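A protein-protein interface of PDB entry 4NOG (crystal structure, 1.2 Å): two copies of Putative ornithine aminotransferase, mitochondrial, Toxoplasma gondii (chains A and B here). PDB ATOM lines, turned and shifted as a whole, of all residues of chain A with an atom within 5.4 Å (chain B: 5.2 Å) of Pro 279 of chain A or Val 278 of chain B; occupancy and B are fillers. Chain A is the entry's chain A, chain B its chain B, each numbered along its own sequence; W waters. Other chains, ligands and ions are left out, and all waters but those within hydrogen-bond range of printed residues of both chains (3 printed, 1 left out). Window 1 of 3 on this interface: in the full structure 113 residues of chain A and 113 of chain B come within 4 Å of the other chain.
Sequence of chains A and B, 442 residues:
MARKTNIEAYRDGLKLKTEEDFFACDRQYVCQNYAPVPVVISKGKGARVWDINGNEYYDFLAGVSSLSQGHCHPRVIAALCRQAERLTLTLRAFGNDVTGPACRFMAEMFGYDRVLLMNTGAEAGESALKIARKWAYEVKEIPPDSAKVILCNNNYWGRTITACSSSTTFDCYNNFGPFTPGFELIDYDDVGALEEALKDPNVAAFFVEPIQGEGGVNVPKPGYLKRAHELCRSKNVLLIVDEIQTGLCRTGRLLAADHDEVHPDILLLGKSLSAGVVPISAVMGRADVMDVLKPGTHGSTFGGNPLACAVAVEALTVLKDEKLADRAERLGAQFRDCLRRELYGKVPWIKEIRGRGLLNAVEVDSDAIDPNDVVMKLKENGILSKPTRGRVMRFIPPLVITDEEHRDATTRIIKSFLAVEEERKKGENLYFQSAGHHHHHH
N of Asn 119 of chain A is in hydrogen-bond range of OG of Ser 281 of chain A, at 3.4 Å.
O of Thr 120 of chain A is in hydrogen-bond range of OG of Ser 281 of chain A.
The side-chain hydroxyl (OG) of Ser 274 of chain A sits at hydrogen-bond distance from the backbone carbonyl oxygen (O) of Val 278 of chain A (2.7 Å).
The side-chain amide oxygen (OD1) of Asn 119 of chain B sits close to the backbone carbonyl oxygen (O) of Phe 302 of chain B (3.3 Å).
The side-chain hydroxyl (OG) of Ser 274 of chain B is in hydrogen-bond range of the backbone NH (N) of Val 277 of chain B (3.4 Å).
O of Val 278 of chain B is in hydrogen-bond range of OG of Ser 274 of chain B (2.7 Å).
Water W2 bridges the backbone carbonyl oxygen of Val 277 of chain B (2.8 Å) and the side-chain amide oxygen of Asn 305 of chain A (2.9 Å).
Water W3 bridges O of Val 277 of chain A (2.8 Å) and OD1 of Asn 305 of chain B (2.9 Å).
Water W1 lies within hydrogen-bond range of the side-chain amide oxygen of Asn 305 of chain B (3.1 Å) and the backbone carbonyl oxygen of Val 277 of chain A (3.2 Å).
Ser 274 of chain A touches Phe 302 of chain B, and with the chains exchanged Phe 302 of chain A touches Ser 274 of chain B.
Val 278 of chain A touches Phe 302 of chain B, and with the chains exchanged Phe 302 of chain A touches Val 278 of chain B.
Pro 279 of chain A touches Val 278 of chain B, but with the chains exchanged Val 278 of chain A does not touch Pro 279 of chain B (5.3 Å).
Pro 279 of chain A touches Phe 302 of chain B, and with the chains exchanged Phe 302 of chain A touches Pro 279 of chain B.
Of the 12 pairs that touch across the chains among the printed residues, 9 have their exchanged pair printed and touching as well.
CG2 of Thr 120 of chain A touches ND2 of Asn 119 of chain B, 3.5 Å away.
OG of Ser 274 of chain A touches CZ of Phe 302 of chain B, 3.7 Å away.
Val 278 of chain B touches Val 278 of chain A.
Val 278 of chain A touches Phe 302 of chain B (C to CE2, 3.9 Å).
CG of Pro 279 of chain A touches OD1 of Asn 119 of chain B, at 3.8 Å.
CD of Pro 279 of chain A touches CG2 of Val 278 of chain B, at 3.8 Å.
CZ of Phe 302 of chain A touches OG of Ser 274 of chain B, at 3.7 Å.
Phe 302 of chain A touches Gly 276 of chain B.
Val 278 of chain B touches Phe 302 of chain A (C to CE1, 3.9 Å).
CB of Pro 279 of chain B touches CG of Phe 302 of chain A, at 3.8 Å.
Printed residues of chain B that touch a printed residue of chain A: Asn 119, Ser 274, Gly 276, Val 278, Pro 279 and Phe 302.
Hydrophobic or aromatic side chains of chain B within 4 Å of the printed part of chain A: Val 278, Pro 279 and Phe 302.
Of the 12 printed residues of chain A, 6 touch a printed residue of chain B.
Hydrophobic or aromatic side chains of chain A within 4 Å of the printed part of chain B: Val 278, Pro 279 and Phe 302.
Among the printed residues, 12 pairs touch across the chains.
Of the printed residues of chain B, Thr 120 of chain A touches Asn 119.
Of the printed residues of chain B, Ser 274 of chain A touches Phe 302.
Of the printed residues of chain B, Pro 279 of chain A touches Asn 119, Val 278 and Phe 302.
Printed residues of chain A within 4 Å of Asn 119 of chain B: Thr 120 and Pro 279.
Printed residues of chain A within 4 Å of Val 278 of chain B: Val 278, Pro 279 and Phe 302.
Of the printed residues of chain A, Pro 279 of chain B touches Asn 119 and Phe 302.
Of the printed residues of chain A, Phe 302 of chain B touches Ser 274, Val 278 and Pro 279.
The nearest printed residue of chain A that does not touch Val 278 of chain B is Val 277 of chain A (5.3 Å).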
ATOM      1  N   MET A 118     -17.477  -3.717  12.392  1.00  0.00           N
ATOM      2  CA  MET A 118     -17.070  -2.516  11.635  1.00  0.00           C
ATOM      3  C   MET A 118     -15.744  -2.064  12.203  1.00  0.00           C
ATOM      4  O   MET A 118     -15.082  -2.797  12.917  1.00  0.00           O
ATOM      5  CB  MET A 118     -18.131  -1.440  11.630  1.00  0.00           C
ATOM      6  CG  MET A 118     -19.474  -1.820  10.987  1.00  0.00           C
ATOM      7  SD  MET A 118     -19.428  -2.198   9.232  1.00  0.00           S
ATOM      8  CE  MET A 118     -19.313  -0.567   8.585  1.00  0.00           C
ATOM      9  N   ASN A 119     -15.290  -0.858  11.807  1.00  0.00           N
ATOM     10  CA  ASN A 119     -13.953  -0.431  12.182  1.00  0.00           C
ATOM     11  C   ASN A 119     -13.963   0.634  13.259  1.00  0.00           C
ATOM     12  O   ASN A 119     -13.205   0.524  14.159  1.00  0.00           O
ATOM     13  CB  ASN A 119     -13.190   0.067  10.936  1.00  0.00           C
ATOM     14  CG  ASN A 119     -13.231  -1.010   9.863  1.00  0.00           C
ATOM     15  OD1 ASN A 119     -12.495  -1.958   9.911  1.00  0.00           O
ATOM     16  ND2 ASN A 119     -14.159  -0.874   8.929  1.00  0.00           N
ATOM     17  N   THR A 120     -14.796   1.627  13.155  1.00  0.00           N
ATOM     18  CA  THR A 120     -14.781   2.745  14.098  1.00  0.00           C
ATOM     19  C   THR A 120     -16.102   2.850  14.827  1.00  0.00           C
ATOM     20  O   THR A 120     -17.108   2.274  14.421  1.00  0.00           O
ATOM     21  CB  THR A 120     -14.485   4.066  13.377  1.00  0.00           C
ATOM     22  OG1 THR A 120     -15.587   4.391  12.536  1.00  0.00           O
ATOM     23  CG2 THR A 120     -13.224   3.984  12.562  1.00  0.00           C
ATOM     24  N   SER A 274     -10.490  -3.506  21.098  1.00  0.00           N
ATOM     25  CA  SER A 274      -9.183  -3.891  20.536  1.00  0.00           C
ATOM     26  C   SER A 274      -7.998  -3.585  21.464  1.00  0.00           C
ATOM     27  O   SER A 274      -6.843  -3.671  21.041  1.00  0.00           O
ATOM     28  CB  SER A 274      -8.928  -3.107  19.260  1.00  0.00           C
ATOM     29  OG  SER A 274      -8.726  -1.757  19.581  1.00  0.00           O
ATOM     30  N   VAL A 277      -5.374  -1.181  19.977  1.00  0.00           N
ATOM     31  CA  VAL A 277      -4.329  -1.627  19.081  1.00  0.00           C
ATOM     32  C   VAL A 277      -4.701  -1.390  17.618  1.00  0.00           C
ATOM     33  O   VAL A 277      -3.868  -0.916  16.848  1.00  0.00           O
ATOM     34  CB  VAL A 277      -3.950  -3.093  19.405  1.00  0.00           C
ATOM     35  CG1 VAL A 277      -2.972  -3.671  18.391  1.00  0.00           C
ATOM     36  CG2 VAL A 277      -3.368  -3.165  20.808  1.00  0.00           C
ATOM     37  N   VAL A 278      -5.945  -1.687  17.255  1.00  0.00           N
ATOM     38  CA  VAL A 278      -6.403  -1.472  15.886  1.00  0.00           C
ATOM     39  C   VAL A 278      -7.881  -1.087  15.975  1.00  0.00           C
ATOM     40  O   VAL A 278      -8.593  -1.554  16.875  1.00  0.00           O
ATOM     41  CB  VAL A 278      -6.177  -2.690  14.998  1.00  0.00           C
ATOM     42  CG1 VAL A 278      -4.705  -3.062  14.761  1.00  0.00           C
ATOM     43  CG2 VAL A 278      -6.891  -3.875  15.534  1.00  0.00           C
ATOM     44  N   PRO A 279      -8.411  -0.359  15.015  1.00  0.00           N
ATOM     45  CA  PRO A 279      -9.799   0.023  15.084  1.00  0.00           C
ATOM     46  C   PRO A 279     -10.736  -1.122  14.751  1.00  0.00           C
ATOM     47  O   PRO A 279     -10.705  -1.613  13.628  1.00  0.00           O
ATOM     48  CB  PRO A 279      -9.938   1.170  14.065  1.00  0.00           C
ATOM     49  CG  PRO A 279      -8.639   1.297  13.430  1.00  0.00           C
ATOM     50  CD  PRO A 279      -7.668   0.365  13.965  1.00  0.00           C
ATOM     51  N   ILE A 280     -11.529  -1.564  15.725  1.00  0.00           N
ATOM     52  CA  ILE A 280     -12.607  -2.553  15.465  1.00  0.00           C
ATOM     53  C   ILE A 280     -13.781  -2.191  16.373  1.00  0.00           C
ATOM     54  O   ILE A 280     -13.591  -1.932  17.556  1.00  0.00           O
ATOM     55  CB  ILE A 280     -12.163  -4.046  15.612  1.00  0.00           C
ATOM     56  CG1 ILE A 280     -13.346  -4.993  15.644  1.00  0.00           C
ATOM     57  CG2 ILE A 280     -11.276  -4.245  16.769  1.00  0.00           C
ATOM     58  CD1 ILE A 280     -12.961  -6.474  15.371  1.00  0.00           C
ATOM     59  N   SER A 281     -14.951  -2.182  15.812  1.00  0.00           N
ATOM     60  CA  SER A 281     -16.220  -1.868  16.480  1.00  0.00           C
ATOM     61  C   SER A 281     -17.192  -2.983  16.197  1.00  0.00           C
ATOM     62  O   SER A 281     -17.003  -3.760  15.259  1.00  0.00           O
ATOM     63  CB  SER A 281     -16.693  -0.497  16.076  1.00  0.00           C
ATOM     64  OG  SER A 281     -17.076  -0.503  14.730  1.00  0.00           O
ATOM     65  N   PHE A 302     -12.547  -3.262   5.571  1.00  0.00           N
ATOM     66  CA  PHE A 302     -11.787  -3.832   6.680  1.00  0.00           C
ATOM     67  C   PHE A 302     -12.649  -4.418   7.791  1.00  0.00           C
ATOM     68  O   PHE A 302     -12.128  -5.031   8.710  1.00  0.00           O
ATOM     69  CB  PHE A 302     -10.806  -2.760   7.252  1.00  0.00           C
ATOM     70  CG  PHE A 302      -9.585  -2.545   6.399  1.00  0.00           C
ATOM     71  CD1 PHE A 302      -8.436  -3.256   6.627  1.00  0.00           C
ATOM     72  CD2 PHE A 302      -9.572  -1.547   5.420  1.00  0.00           C
ATOM     73  CE1 PHE A 302      -7.325  -3.066   5.820  1.00  0.00           C
ATOM     74  CE2 PHE A 302      -8.436  -1.329   4.650  1.00  0.00           C
ATOM     75  CZ  PHE A 302      -7.322  -2.098   4.842  1.00  0.00           C
ATOM     76  N   ASN A 305     -11.966  -7.977   9.591  1.00  0.00           N
ATOM     77  CA  ASN A 305     -10.711  -8.553   9.091  1.00  0.00           C
ATOM     78  C   ASN A 305     -10.122  -9.446  10.133  1.00  0.00           C
ATOM     79  O   ASN A 305     -10.279  -9.207  11.335  1.00  0.00           O
ATOM     80  CB  ASN A 305      -9.771  -7.447   8.642  1.00  0.00           C
ATOM     81  CG  ASN A 305      -9.157  -6.653   9.789  1.00  0.00           C
ATOM     82  OD1 ASN A 305      -8.204  -7.112  10.415  1.00  0.00           O
ATOM     83  ND2 ASN A 305      -9.691  -5.464  10.045  1.00  0.00           N
ATOM     84  N   ALA A 308      -7.832  -7.868  13.118  1.00  0.00           N
ATOM     85  CA  ALA A 308      -8.570  -7.177  14.169  1.00  0.00           C
ATOM     86  C   ALA A 308      -9.374  -8.196  14.986  1.00  0.00           C
ATOM     87  O   ALA A 308      -9.556  -8.031  16.202  1.00  0.00           O
ATOM     88  CB  ALA A 308      -9.484  -6.154  13.561  1.00  0.00           C
ATOM     89  N   ASN B 119      -9.719   6.371   9.323  1.00  0.00           N
ATOM     90  CA  ASN B 119      -9.531   4.934   9.390  1.00  0.00           C
ATOM     91  C   ASN B 119     -10.025   4.203   8.180  1.00  0.00           C
ATOM     92  O   ASN B 119      -9.296   3.352   7.685  1.00  0.00           O
ATOM     93  CB  ASN B 119     -10.193   4.408  10.654  1.00  0.00           C
ATOM     94  CG  ASN B 119      -9.751   5.180  11.887  1.00  0.00           C
ATOM     95  OD1 ASN B 119      -8.710   4.964  12.404  1.00  0.00           O
ATOM     96  ND2 ASN B 119     -10.549   6.161  12.261  1.00  0.00           N
ATOM     97  N   SER B 274      -2.283   0.862   3.786  1.00  0.00           N
ATOM     98  CA  SER B 274      -1.766   0.062   4.910  1.00  0.00           C
ATOM     99  C   SER B 274      -1.275  -1.320   4.479  1.00  0.00           C
ATOM    100  O   SER B 274      -1.037  -2.175   5.332  1.00  0.00           O
ATOM    101  CB  SER B 274      -2.865  -0.149   5.907  1.00  0.00           C
ATOM    102  OG  SER B 274      -3.865  -0.973   5.371  1.00  0.00           O
ATOM    103  N   GLY B 276      -3.152  -3.502   3.560  1.00  0.00           N
ATOM    104  CA  GLY B 276      -4.181  -4.427   3.995  1.00  0.00           C
ATOM    105  C   GLY B 276      -3.988  -4.881   5.442  1.00  0.00           C
ATOM    106  O   GLY B 276      -4.664  -5.851   5.839  1.00  0.00           O
ATOM    107  N   VAL B 277      -3.130  -4.226   6.211  1.00  0.00           N
ATOM    108  CA  VAL B 277      -2.835  -4.706   7.514  1.00  0.00           C
ATOM    109  C   VAL B 277      -3.754  -4.081   8.584  1.00  0.00           C
ATOM    110  O   VAL B 277      -4.211  -4.813   9.469  1.00  0.00           O
ATOM    111  CB  VAL B 277      -1.323  -4.506   7.800  1.00  0.00           C
ATOM    112  CG1 VAL B 277      -0.944  -4.843   9.236  1.00  0.00           C
ATOM    113  CG2 VAL B 277      -0.497  -5.336   6.817  1.00  0.00           C
ATOM    114  N   VAL B 278      -4.063  -2.796   8.452  1.00  0.00           N
ATOM    115  CA  VAL B 278      -4.943  -2.169   9.407  1.00  0.00           C
ATOM    116  C   VAL B 278      -5.650  -1.062   8.674  1.00  0.00           C
ATOM    117  O   VAL B 278      -5.122  -0.499   7.702  1.00  0.00           O
ATOM    118  CB  VAL B 278      -4.142  -1.598  10.612  1.00  0.00           C
ATOM    119  CG1 VAL B 278      -3.116  -0.549  10.163  1.00  0.00           C
ATOM    120  CG2 VAL B 278      -4.992  -1.061  11.676  1.00  0.00           C
ATOM    121  N   PRO B 279      -6.821  -0.671   9.128  1.00  0.00           N
ATOM    122  CA  PRO B 279      -7.530   0.351   8.391  1.00  0.00           C
ATOM    123  C   PRO B 279      -6.931   1.741   8.623  1.00  0.00           C
ATOM    124  O   PRO B 279      -6.943   2.216   9.746  1.00  0.00           O
ATOM    125  CB  PRO B 279      -8.958   0.275   8.923  1.00  0.00           C
ATOM    126  CG  PRO B 279      -8.987  -0.706   9.966  1.00  0.00           C
ATOM    127  CD  PRO B 279      -7.670  -1.316  10.138  1.00  0.00           C
ATOM    128  N   ILE B 280      -6.393   2.367   7.579  1.00  0.00           N
ATOM    129  CA  ILE B 280      -5.990   3.758   7.598  1.00  0.00           C
ATOM    130  C   ILE B 280      -6.289   4.403   6.263  1.00  0.00           C
ATOM    131  O   ILE B 280      -5.957   3.854   5.235  1.00  0.00           O
ATOM    132  CB  ILE B 280      -4.505   3.979   8.074  1.00  0.00           C
ATOM    133  CG1 ILE B 280      -4.019   5.408   7.847  1.00  0.00           C
ATOM    134  CG2 ILE B 280      -3.537   2.995   7.498  1.00  0.00           C
ATOM    135  CD1 ILE B 280      -2.733   5.786   8.637  1.00  0.00           C
ATOM    136  N   PHE B 302      -9.354   6.680  16.526  1.00  0.00           N
ATOM    137  CA  PHE B 302      -8.185   5.978  15.997  1.00  0.00           C
ATOM    138  C   PHE B 302      -7.481   6.684  14.828  1.00  0.00           C
ATOM    139  O   PHE B 302      -6.431   6.244  14.414  1.00  0.00           O
ATOM    140  CB  PHE B 302      -8.533   4.510  15.592  1.00  0.00           C
ATOM    141  CG  PHE B 302      -8.718   3.584  16.770  1.00  0.00           C
ATOM    142  CD1 PHE B 302      -9.937   3.467  17.405  1.00  0.00           C
ATOM    143  CD2 PHE B 302      -7.657   2.868  17.246  1.00  0.00           C
ATOM    144  CE1 PHE B 302     -10.135   2.601  18.468  1.00  0.00           C
ATOM    145  CE2 PHE B 302      -7.840   2.002  18.317  1.00  0.00           C
ATOM    146  CZ  PHE B 302      -9.069   1.891  18.921  1.00  0.00           C
ATOM    147  N   ASN B 305      -3.531   7.109  14.480  1.00  0.00           N
ATOM    148  CA  ASN B 305      -2.834   6.414  15.561  1.00  0.00           C
ATOM    149  C   ASN B 305      -1.420   6.041  15.134  1.00  0.00           C
ATOM    150  O   ASN B 305      -1.199   5.739  13.936  1.00  0.00           O
ATOM    151  CB  ASN B 305      -3.641   5.234  16.058  1.00  0.00           C
ATOM    152  CG  ASN B 305      -3.689   4.100  15.072  1.00  0.00           C
ATOM    153  OD1 ASN B 305      -2.739   3.287  15.027  1.00  0.00           O
ATOM    154  ND2 ASN B 305      -4.742   4.031  14.308  1.00  0.00           N
ATOM    155  N   ALA B 308      -0.858   2.614  12.971  1.00  0.00           N
ATOM    156  CA  ALA B 308      -1.288   2.662  11.599  1.00  0.00           C
ATOM    157  C   ALA B 308      -0.355   3.566  10.820  1.00  0.00           C
ATOM    158  O   ALA B 308      -0.051   3.306   9.639  1.00  0.00           O
ATOM    159  CB  ALA B 308      -2.703   3.163  11.518  1.00  0.00           C
ATOM    160  N   VAL B 311       2.800   1.611   9.932  1.00  0.00           N
ATOM    161  CA  VAL B 311       2.444   0.673   8.890  1.00  0.00           C
ATOM    162  C   VAL B 311       2.302   1.349   7.555  1.00  0.00           C
ATOM    163  O   VAL B 311       2.834   0.855   6.531  1.00  0.00           O
ATOM    164  CB  VAL B 311       1.141  -0.081   9.278  1.00  0.00           C
ATOM    165  CG1 VAL B 311       0.594  -0.844   8.084  1.00  0.00           C
ATOM    166  CG2 VAL B 311       1.390  -1.023  10.433  1.00  0.00           C
HETATM  167  O   HOH W   1      -4.243   2.186  17.505  1.00  0.00           O
HETATM  168  O   HOH W   2      -6.459  -4.901  11.125  1.00  0.00           O
HETATM  169  O   HOH W   3      -3.798   0.611  14.464  1.00  0.00           O
